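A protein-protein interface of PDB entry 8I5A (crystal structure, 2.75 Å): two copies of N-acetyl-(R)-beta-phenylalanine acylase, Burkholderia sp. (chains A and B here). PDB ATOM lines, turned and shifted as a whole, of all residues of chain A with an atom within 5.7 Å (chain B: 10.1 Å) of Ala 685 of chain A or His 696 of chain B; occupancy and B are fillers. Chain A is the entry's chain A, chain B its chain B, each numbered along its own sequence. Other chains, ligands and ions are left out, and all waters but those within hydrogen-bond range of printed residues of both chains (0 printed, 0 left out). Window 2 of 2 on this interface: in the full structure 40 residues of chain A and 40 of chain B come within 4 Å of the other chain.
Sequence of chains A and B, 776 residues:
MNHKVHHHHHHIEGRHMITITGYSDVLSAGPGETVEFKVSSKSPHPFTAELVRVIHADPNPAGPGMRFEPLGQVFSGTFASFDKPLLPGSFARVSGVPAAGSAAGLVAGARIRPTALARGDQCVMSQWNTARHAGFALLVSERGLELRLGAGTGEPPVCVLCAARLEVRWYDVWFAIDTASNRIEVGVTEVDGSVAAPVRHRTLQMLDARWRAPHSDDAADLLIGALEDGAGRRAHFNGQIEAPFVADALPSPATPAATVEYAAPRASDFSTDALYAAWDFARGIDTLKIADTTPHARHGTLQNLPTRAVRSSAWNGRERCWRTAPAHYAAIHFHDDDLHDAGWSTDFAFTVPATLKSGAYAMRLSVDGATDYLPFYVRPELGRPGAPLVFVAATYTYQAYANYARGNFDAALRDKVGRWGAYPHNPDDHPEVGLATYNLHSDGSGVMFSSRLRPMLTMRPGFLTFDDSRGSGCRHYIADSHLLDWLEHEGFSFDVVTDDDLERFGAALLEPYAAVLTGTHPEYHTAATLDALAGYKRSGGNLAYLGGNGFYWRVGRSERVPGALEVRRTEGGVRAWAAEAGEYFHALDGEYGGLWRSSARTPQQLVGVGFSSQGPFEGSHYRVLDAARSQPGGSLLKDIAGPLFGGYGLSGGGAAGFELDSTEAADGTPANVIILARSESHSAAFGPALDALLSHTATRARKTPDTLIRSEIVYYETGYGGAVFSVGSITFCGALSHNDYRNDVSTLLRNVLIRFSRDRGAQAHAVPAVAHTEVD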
ATOM      1  N   GLN A 614       7.169  33.442   7.179  1.00  0.00           N
ATOM      2  CA  GLN A 614       6.684  34.304   8.245  1.00  0.00           C
ATOM      3  C   GLN A 614       7.887  34.865   8.976  1.00  0.00           C
ATOM      4  O   GLN A 614       8.872  34.157   9.201  1.00  0.00           O
ATOM      5  CB  GLN A 614       5.772  33.547   9.236  1.00  0.00           C
ATOM      6  CG  GLN A 614       5.819  34.059  10.668  1.00  0.00           C
ATOM      7  CD  GLN A 614       6.626  33.160  11.582  1.00  0.00           C
ATOM      8  OE1 GLN A 614       6.524  31.930  11.517  1.00  0.00           O
ATOM      9  NE2 GLN A 614       7.465  33.772  12.424  1.00  0.00           N
ATOM     10  N   GLY A 615       7.811  36.145   9.317  1.00  0.00           N
ATOM     11  CA  GLY A 615       8.831  36.776  10.108  1.00  0.00           C
ATOM     12  C   GLY A 615       8.192  37.719  11.092  1.00  0.00           C
ATOM     13  O   GLY A 615       6.997  37.632  11.399  1.00  0.00           O
ATOM     14  N   PRO A 616       8.989  38.629  11.624  1.00  0.00           N
ATOM     15  CA  PRO A 616       8.439  39.687  12.484  1.00  0.00           C
ATOM     16  C   PRO A 616       7.628  40.693  11.670  1.00  0.00           C
ATOM     17  O   PRO A 616       7.537  40.569  10.442  1.00  0.00           O
ATOM     18  CB  PRO A 616       9.691  40.328  13.104  1.00  0.00           C
ATOM     19  CG  PRO A 616      10.872  39.499  12.649  1.00  0.00           C
ATOM     20  CD  PRO A 616      10.445  38.749  11.434  1.00  0.00           C
ATOM     21  N   GLU A 618       7.840  43.358   9.867  1.00  0.00           N
ATOM     22  CA  GLU A 618       8.765  44.199   9.110  1.00  0.00           C
ATOM     23  C   GLU A 618       8.592  43.903   7.624  1.00  0.00           C
ATOM     24  O   GLU A 618       8.407  42.748   7.236  1.00  0.00           O
ATOM     25  CB  GLU A 618      10.239  44.009   9.525  1.00  0.00           C
ATOM     26  CG  GLU A 618      10.608  42.641  10.087  1.00  0.00           C
ATOM     27  CD  GLU A 618      12.035  42.573  10.625  1.00  0.00           C
ATOM     28  OE1 GLU A 618      12.979  42.596   9.811  1.00  0.00           O
ATOM     29  OE2 GLU A 618      12.212  42.484  11.859  1.00  0.00           O
ATOM     30  N   SER A 683      14.661  40.304   6.548  1.00  0.00           N
ATOM     31  CA  SER A 683      15.639  40.099   7.607  1.00  0.00           C
ATOM     32  C   SER A 683      15.861  38.606   7.859  1.00  0.00           C
ATOM     33  O   SER A 683      15.044  37.756   7.494  1.00  0.00           O
ATOM     34  CB  SER A 683      15.196  40.788   8.889  1.00  0.00           C
ATOM     35  OG  SER A 683      14.516  39.903   9.745  1.00  0.00           O
ATOM     36  N   ALA A 684      16.972  38.292   8.532  1.00  0.00           N
ATOM     37  CA  ALA A 684      17.302  36.898   8.794  1.00  0.00           C
ATOM     38  C   ALA A 684      16.266  36.221   9.667  1.00  0.00           C
ATOM     39  O   ALA A 684      16.220  34.986   9.706  1.00  0.00           O
ATOM     40  CB  ALA A 684      18.667  36.787   9.455  1.00  0.00           C
ATOM     41  N   ALA A 685      15.431  37.002  10.361  1.00  0.00           N
ATOM     42  CA  ALA A 685      14.383  36.461  11.219  1.00  0.00           C
ATOM     43  C   ALA A 685      13.257  35.780  10.443  1.00  0.00           C
ATOM     44  O   ALA A 685      12.452  35.071  11.056  1.00  0.00           O
ATOM     45  CB  ALA A 685      13.797  37.577  12.080  1.00  0.00           C
ATOM     46  N   PHE A 686      13.183  35.959   9.123  1.00  0.00           N
ATOM     47  CA  PHE A 686      12.136  35.318   8.332  1.00  0.00           C
ATOM     48  C   PHE A 686      12.482  33.851   8.100  1.00  0.00           C
ATOM     49  O   PHE A 686      13.575  33.533   7.626  1.00  0.00           O
ATOM     50  CB  PHE A 686      11.936  36.048   6.999  1.00  0.00           C
ATOM     51  CG  PHE A 686      11.026  37.229   7.109  1.00  0.00           C
ATOM     52  CD1 PHE A 686      11.494  38.426   7.625  1.00  0.00           C
ATOM     53  CD2 PHE A 686       9.695  37.133   6.738  1.00  0.00           C
ATOM     54  CE1 PHE A 686      10.655  39.517   7.756  1.00  0.00           C
ATOM     55  CE2 PHE A 686       8.850  38.216   6.856  1.00  0.00           C
ATOM     56  CZ  PHE A 686       9.330  39.416   7.369  1.00  0.00           C
ATOM     57  N   GLY A 687      11.545  32.964   8.442  1.00  0.00           N
ATOM     58  CA  GLY A 687      11.735  31.535   8.312  1.00  0.00           C
ATOM     59  C   GLY A 687      10.627  30.868   7.520  1.00  0.00           C
ATOM     60  O   GLY A 687       9.659  31.510   7.097  1.00  0.00           O
ATOM     61  N   PRO A 688      10.738  29.557   7.317  1.00  0.00           N
ATOM     62  CA  PRO A 688       9.776  28.859   6.454  1.00  0.00           C
ATOM     63  C   PRO A 688       8.515  28.397   7.169  1.00  0.00           C
ATOM     64  O   PRO A 688       8.519  28.027   8.343  1.00  0.00           O
ATOM     65  CB  PRO A 688      10.590  27.659   5.960  1.00  0.00           C
ATOM     66  CG  PRO A 688      11.582  27.435   7.039  1.00  0.00           C
ATOM     67  CD  PRO A 688      11.945  28.752   7.575  1.00  0.00           C
ATOM     68  N   LEU A 690       6.068  25.884   8.328  1.00  0.00           N
ATOM     69  CA  LEU A 690       6.422  24.503   8.637  1.00  0.00           C
ATOM     70  C   LEU A 690       5.657  23.512   7.768  1.00  0.00           C
ATOM     71  O   LEU A 690       6.219  22.496   7.337  1.00  0.00           O
ATOM     72  CB  LEU A 690       6.180  24.212  10.120  1.00  0.00           C
ATOM     73  CG  LEU A 690       7.127  24.978  11.053  1.00  0.00           C
ATOM     74  CD1 LEU A 690       6.907  24.604  12.507  1.00  0.00           C
ATOM     75  CD2 LEU A 690       8.574  24.776  10.648  1.00  0.00           C
ATOM     76  N   GLY B 687      19.777  19.930  12.092  1.00  0.00           N
ATOM     77  CA  GLY B 687      18.596  20.721  12.317  1.00  0.00           C
ATOM     78  C   GLY B 687      17.598  20.040  13.230  1.00  0.00           C
ATOM     79  O   GLY B 687      17.820  18.935  13.733  1.00  0.00           O
ATOM     80  N   PRO B 688      16.477  20.712  13.474  1.00  0.00           N
ATOM     81  CA  PRO B 688      15.466  20.206  14.403  1.00  0.00           C
ATOM     82  C   PRO B 688      14.440  19.292  13.747  1.00  0.00           C
ATOM     83  O   PRO B 688      14.152  19.375  12.549  1.00  0.00           O
ATOM     84  CB  PRO B 688      14.809  21.499  14.892  1.00  0.00           C
ATOM     85  CG  PRO B 688      14.920  22.423  13.711  1.00  0.00           C
ATOM     86  CD  PRO B 688      16.076  21.995  12.870  1.00  0.00           C
ATOM     87  N   ALA B 689      13.909  18.377  14.562  1.00  0.00           N
ATOM     88  CA  ALA B 689      12.824  17.503  14.121  1.00  0.00           C
ATOM     89  C   ALA B 689      11.508  18.279  14.032  1.00  0.00           C
ATOM     90  O   ALA B 689      11.065  18.890  15.016  1.00  0.00           O
ATOM     91  CB  ALA B 689      12.673  16.322  15.073  1.00  0.00           C
ATOM     92  N   LEU B 690      10.870  18.229  12.853  1.00  0.00           N
ATOM     93  CA  LEU B 690       9.747  19.114  12.559  1.00  0.00           C
ATOM     94  C   LEU B 690       8.593  18.933  13.541  1.00  0.00           C
ATOM     95  O   LEU B 690       7.967  19.918  13.946  1.00  0.00           O
ATOM     96  CB  LEU B 690       9.279  18.886  11.125  1.00  0.00           C
ATOM     97  CG  LEU B 690      10.298  19.404  10.108  1.00  0.00           C
ATOM     98  CD1 LEU B 690       9.730  19.415   8.687  1.00  0.00           C
ATOM     99  CD2 LEU B 690      10.798  20.795  10.520  1.00  0.00           C
ATOM    100  N   ALA B 692       8.576  18.483  16.565  1.00  0.00           N
ATOM    101  CA  ALA B 692       8.845  19.181  17.814  1.00  0.00           C
ATOM    102  C   ALA B 692       8.673  20.708  17.702  1.00  0.00           C
ATOM    103  O   ALA B 692       9.036  21.418  18.643  1.00  0.00           O
ATOM    104  CB  ALA B 692      10.257  18.838  18.313  1.00  0.00           C
ATOM    105  N   LEU B 693       8.103  21.224  16.603  1.00  0.00           N
ATOM    106  CA  LEU B 693       8.085  22.658  16.315  1.00  0.00           C
ATOM    107  C   LEU B 693       6.659  23.193  16.192  1.00  0.00           C
ATOM    108  O   LEU B 693       5.835  22.633  15.458  1.00  0.00           O
ATOM    109  CB  LEU B 693       8.864  22.973  15.017  1.00  0.00           C
ATOM    110  CG  LEU B 693      10.395  22.811  15.041  1.00  0.00           C
ATOM    111  CD1 LEU B 693      11.025  23.353  13.795  1.00  0.00           C
ATOM    112  CD2 LEU B 693      11.033  23.451  16.280  1.00  0.00           C
ATOM    113  N   LEU B 694       6.387  24.307  16.882  1.00  0.00           N
ATOM    114  CA  LEU B 694       5.183  25.092  16.646  1.00  0.00           C
ATOM    115  C   LEU B 694       5.401  26.150  15.574  1.00  0.00           C
ATOM    116  O   LEU B 694       4.469  26.477  14.826  1.00  0.00           O
ATOM    117  CB  LEU B 694       4.713  25.738  17.941  1.00  0.00           C
ATOM    118  CG  LEU B 694       4.116  24.731  18.918  1.00  0.00           C
ATOM    119  CD1 LEU B 694       4.273  25.208  20.338  1.00  0.00           C
ATOM    120  CD2 LEU B 694       2.651  24.470  18.609  1.00  0.00           C
ATOM    121  N   SER B 695       6.603  26.707  15.506  1.00  0.00           N
ATOM    122  CA  SER B 695       7.012  27.583  14.420  1.00  0.00           C
ATOM    123  C   SER B 695       8.494  27.349  14.184  1.00  0.00           C
ATOM    124  O   SER B 695       9.106  26.482  14.810  1.00  0.00           O
ATOM    125  CB  SER B 695       6.713  29.055  14.724  1.00  0.00           C
ATOM    126  OG  SER B 695       7.568  29.556  15.734  1.00  0.00           O
ATOM    127  N   HIS B 696       9.069  28.108  13.247  1.00  0.00           N
ATOM    128  CA  HIS B 696      10.503  27.998  13.033  1.00  0.00           C
ATOM    129  C   HIS B 696      11.309  28.645  14.149  1.00  0.00           C
ATOM    130  O   HIS B 696      12.534  28.532  14.141  1.00  0.00           O
ATOM    131  CB  HIS B 696      10.883  28.572  11.654  1.00  0.00           C
ATOM    132  CG  HIS B 696      11.042  30.063  11.610  1.00  0.00           C
ATOM    133  ND1 HIS B 696      12.276  30.682  11.652  1.00  0.00           N
ATOM    134  CD2 HIS B 696      10.126  31.058  11.493  1.00  0.00           C
ATOM    135  CE1 HIS B 696      12.114  31.993  11.588  1.00  0.00           C
ATOM    136  NE2 HIS B 696      10.819  32.247  11.491  1.00  0.00           N
ATOM    137  N   THR B 697      10.661  29.266  15.136  1.00  0.00           N
ATOM    138  CA  THR B 697      11.368  29.875  16.257  1.00  0.00           C
ATOM    139  C   THR B 697      10.914  29.348  17.611  1.00  0.00           C
ATOM    140  O   THR B 697      11.368  29.865  18.635  1.00  0.00           O
ATOM    141  CB  THR B 697      11.220  31.408  16.237  1.00  0.00           C
ATOM    142  OG1 THR B 697       9.841  31.770  16.304  1.00  0.00           O
ATOM    143  CG2 THR B 697      11.810  31.999  14.976  1.00  0.00           C
ATOM    144  N   ALA B 698      10.064  28.321  17.658  1.00  0.00           N
ATOM    145  CA  ALA B 698       9.567  27.838  18.945  1.00  0.00           C
ATOM    146  C   ALA B 698       9.239  26.349  18.900  1.00  0.00           C
ATOM    147  O   ALA B 698       8.531  25.883  18.001  1.00  0.00           O
ATOM    148  CB  ALA B 698       8.330  28.627  19.379  1.00  0.00           C
ATOM    149  N   THR B 699       9.745  25.613  19.882  1.00  0.00           N
ATOM    150  CA  THR B 699       9.404  24.212  20.051  1.00  0.00           C
ATOM    151  C   THR B 699       8.052  24.074  20.762  1.00  0.00           C
ATOM    152  O   THR B 699       7.404  25.062  21.119  1.00  0.00           O
ATOM    153  CB  THR B 699      10.525  23.498  20.796  1.00  0.00           C
ATOM    154  OG1 THR B 699      10.370  23.671  22.217  1.00  0.00           O
ATOM    155  CG2 THR B 699      11.872  24.046  20.328  1.00  0.00           C
ATOM    156  N   ARG B 700       7.587  22.830  20.922  1.00  0.00           N
ATOM    157  CA  ARG B 700       6.335  22.586  21.635  1.00  0.00           C
ATOM    158  C   ARG B 700       6.430  23.036  23.092  1.00  0.00           C
ATOM    159  O   ARG B 700       5.417  23.407  23.706  1.00  0.00           O
ATOM    160  CB  ARG B 700       5.964  21.097  21.558  1.00  0.00           C
ATOM    161  CG  ARG B 700       5.345  20.612  20.233  1.00  0.00           C
ATOM    162  CD  ARG B 700       5.097  19.106  20.310  1.00  0.00           C
ATOM    163  NE  ARG B 700       4.420  18.562  19.136  1.00  0.00           N
ATOM    164  CZ  ARG B 700       3.106  18.377  19.052  1.00  0.00           C
ATOM    165  NH1 ARG B 700       2.301  18.679  20.064  1.00  0.00           N
ATOM    166  NH2 ARG B 700       2.584  17.896  17.920  1.00  0.00           N
ATOM    167  N   LYS B 703      10.660  26.671  23.795  1.00  0.00           N
ATOM    168  CA  LYS B 703      12.065  27.057  23.811  1.00  0.00           C
ATOM    169  C   LYS B 703      12.543  27.329  22.392  1.00  0.00           C
ATOM    170  O   LYS B 703      11.823  27.115  21.417  1.00  0.00           O
ATOM    171  CB  LYS B 703      12.939  25.984  24.465  1.00  0.00           C
ATOM    172  CG  LYS B 703      13.335  26.312  25.892  1.00  0.00           C
ATOM    173  CD  LYS B 703      13.490  25.043  26.709  1.00  0.00           C
ATOM    174  CE  LYS B 703      12.173  24.264  26.734  1.00  0.00           C
ATOM    175  NZ  LYS B 703      12.285  22.959  27.466  1.00  0.00           N
ATOM    176  N   THR B 704      13.759  27.841  22.280  1.00  0.00           N
ATOM    177  CA  THR B 704      14.230  28.064  20.920  1.00  0.00           C
ATOM    178  C   THR B 704      14.705  26.742  20.311  1.00  0.00           C
ATOM    179  O   THR B 704      15.021  25.788  21.037  1.00  0.00           O
ATOM    180  CB  THR B 704      15.343  29.130  20.884  1.00  0.00           C
ATOM    181  OG1 THR B 704      16.553  28.635  21.477  1.00  0.00           O
ATOM    182  CG2 THR B 704      14.902  30.400  21.627  1.00  0.00           C
ATOM    183  N   PRO B 705      14.693  26.637  18.981  1.00  0.00           N
ATOM    184  CA  PRO B 705      15.004  25.345  18.340  1.00  0.00           C
ATOM    185  C   PRO B 705      16.426  24.828  18.560  1.00  0.00           C
ATOM    186  O   PRO B 705      16.639  23.610  18.488  1.00  0.00           O
ATOM    187  CB  PRO B 705      14.735  25.630  16.854  1.00  0.00           C
ATOM    188  CG  PRO B 705      13.755  26.767  16.863  1.00  0.00           C
ATOM    189  CD  PRO B 705      14.159  27.619  18.022  1.00  0.00           C
ATOM    190  N   ASP B 706      17.410  25.703  18.790  1.00  0.00           N
ATOM    191  CA  ASP B 706      18.783  25.239  19.009  1.00  0.00           C
ATOM    192  C   ASP B 706      18.926  24.359  20.244  1.00  0.00           C
ATOM    193  O   ASP B 706      19.897  23.599  20.332  1.00  0.00           O
ATOM    194  CB  ASP B 706      19.729  26.423  19.129  1.00  0.00           C
ATOM    195  CG  ASP B 706      19.126  27.544  19.945  1.00  0.00           C
ATOM    196  OD1 ASP B 706      18.336  28.336  19.372  1.00  0.00           O
ATOM    197  OD2 ASP B 706      19.403  27.621  21.169  1.00  0.00           O
ATOM    198  N   THR B 707      18.004  24.453  21.209  1.00  0.00           N
ATOM    199  CA  THR B 707      18.031  23.537  22.345  1.00  0.00           C
ATOM    200  C   THR B 707      17.779  22.096  21.931  1.00  0.00           C
ATOM    201  O   THR B 707      17.949  21.191  22.760  1.00  0.00           O
ATOM    202  CB  THR B 707      16.995  23.929  23.403  1.00  0.00           C
ATOM    203  OG1 THR B 707      15.700  23.464  23.001  1.00  0.00           O
ATOM    204  CG2 THR B 707      16.965  25.437  23.603  1.00  0.00           C
ATOM    205  N   LEU B 708      17.393  21.858  20.676  1.00  0.00           N
ATOM    206  CA  LEU B 708      17.124  20.509  20.211  1.00  0.00           C
ATOM    207  C   LEU B 708      18.353  19.793  19.678  1.00  0.00           C
ATOM    208  O   LEU B 708      18.389  18.561  19.713  1.00  0.00           O
ATOM    209  CB  LEU B 708      16.054  20.537  19.116  1.00  0.00           C
ATOM    210  CG  LEU B 708      14.629  20.843  19.571  1.00  0.00           C
ATOM    211  CD1 LEU B 708      13.716  21.007  18.367  1.00  0.00           C
ATOM    212  CD2 LEU B 708      14.125  19.748  20.468  1.00  0.00           C
ATOM    213  N   ILE B 709      19.371  20.518  19.219  1.00  0.00           N
ATOM    214  CA  ILE B 709      20.515  19.876  18.580  1.00  0.00           C
ATOM    215  C   ILE B 709      21.415  19.321  19.680  1.00  0.00           C
ATOM    216  O   ILE B 709      22.420  19.933  20.062  1.00  0.00           O
ATOM    217  CB  ILE B 709      21.258  20.838  17.639  1.00  0.00           C
ATOM    218  CG1 ILE B 709      20.519  20.970  16.312  1.00  0.00           C
ATOM    219  CG2 ILE B 709      22.588  20.275  17.255  1.00  0.00           C
ATOM    220  CD1 ILE B 709      19.211  21.696  16.349  1.00  0.00           C
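A ring nitrogen (NE2) of His 696 of chain B lies close to the backbone carbonyl oxygen (O) of Ala 685 of chain A, at 3.3 Å. A ring nitrogen (NE2) of His 696 of chain B is in hydrogen-bond range of the backbone NH (N) of Gly 687 of chain A, 3.2 Å away.
The backbone carbonyl oxygen (O) of Gln 614 of chain A lies within hydrogen-bond range of the backbone NH (N) of Gly 687 of chain A (3.0 Å). The backbone NH of Ala 685 of chain A lies close to the side-chain hydroxyl of Ser 683 of chain A (3.1 Å). The backbone NH (N) of Thr 697 of chain B lies close to the side-chain hydroxyl (OG) of Ser 695 of chain B (3.2 Å). The side-chain hydroxyl (OG) of Ser 695 of chain B is in hydrogen-bond range of the backbone NH (N) of Ala 698 of chain B, 3.4 Å away.
Among the printed residues, merely in contact across the chains: Gln 614 of chain A with His 696 of chain B (3.6 Å), Phe 686 of chain A with His 696 of chain B (3.97 Å), Leu 690 of chain A with Leu 693 of chain B (3.6 Å), Leu 690 of chain A with Leu 694 of chain B (3.8 Å) and Leu 690 of chain A with Ser 695 of chain B (3.5 Å).
Of chain B, only His 696 (3.6 Å) comes within 4 Å of Gln 614 of chain A. No residue of chain B comes within 4 Å of Gly 615 of chain A. Glu 618 of chain A touches none of the printed residues of chain B. No residue of chain B comes within 4 Å of Ser 683 of chain A. No residue of chain B comes within 4 Å of Ala 684 of chain A. Of the printed residues of chain B, Ala 685 of chain A touches His 696. Printed residues of chain B within 4 Å of Phe 686 of chain A: His 696. Gly 687 of chain A touches just one residue of chain B: His 696. No residue of chain B comes within 4 Å of Pro 688 of chain A. Printed residues of chain B within 4 Å of Leu 690 of chain A: Leu 693 (3.6 Å), Leu 694 (3.8 Å) and Ser 695 (3.5 Å). Of the printed residues of chain A, Leu 693 of chain B touches Leu 690 (3.6 Å). Of the printed residues of chain A, Leu 694 of chain B touches Leu 690 (3.8 Å). Of the printed residues of chain A, Ser 695 of chain B touches Leu 690 (3.5 Å). Of the printed residues of chain A, His 696 of chain B touches Gln 614 (3.6 Å), Ala 685 (3.1 Å), Phe 686 (3.97 Å) and Gly 687 (3.2 Å). Leu 708 of chain B touches none of the printed residues of chain A. The nearest residue of chain A that does not touch His 696 of chain B is Pro 688 of chain A (4.1 Å).
Hydrophobic or aromatic side chains of chain A within 4 Å of the printed part of chain B: Leu 690. Along chain A the printed residues that touch a printed residue of chain B span positions 614 to 690. Of the 20 printed residues of chain B, 4 touch a printed residue of chain A. Hydrophobic or aromatic side chains of chain B within 4 Å of the printed part of chain A: Leu 693 and His 696. Among the printed residues, no Asp or Glu carboxylate lies within 4 Å of a Lys or Arg side-chain nitrogen of the other chain.
Positions printed for both chains: 687, 688 and 690.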
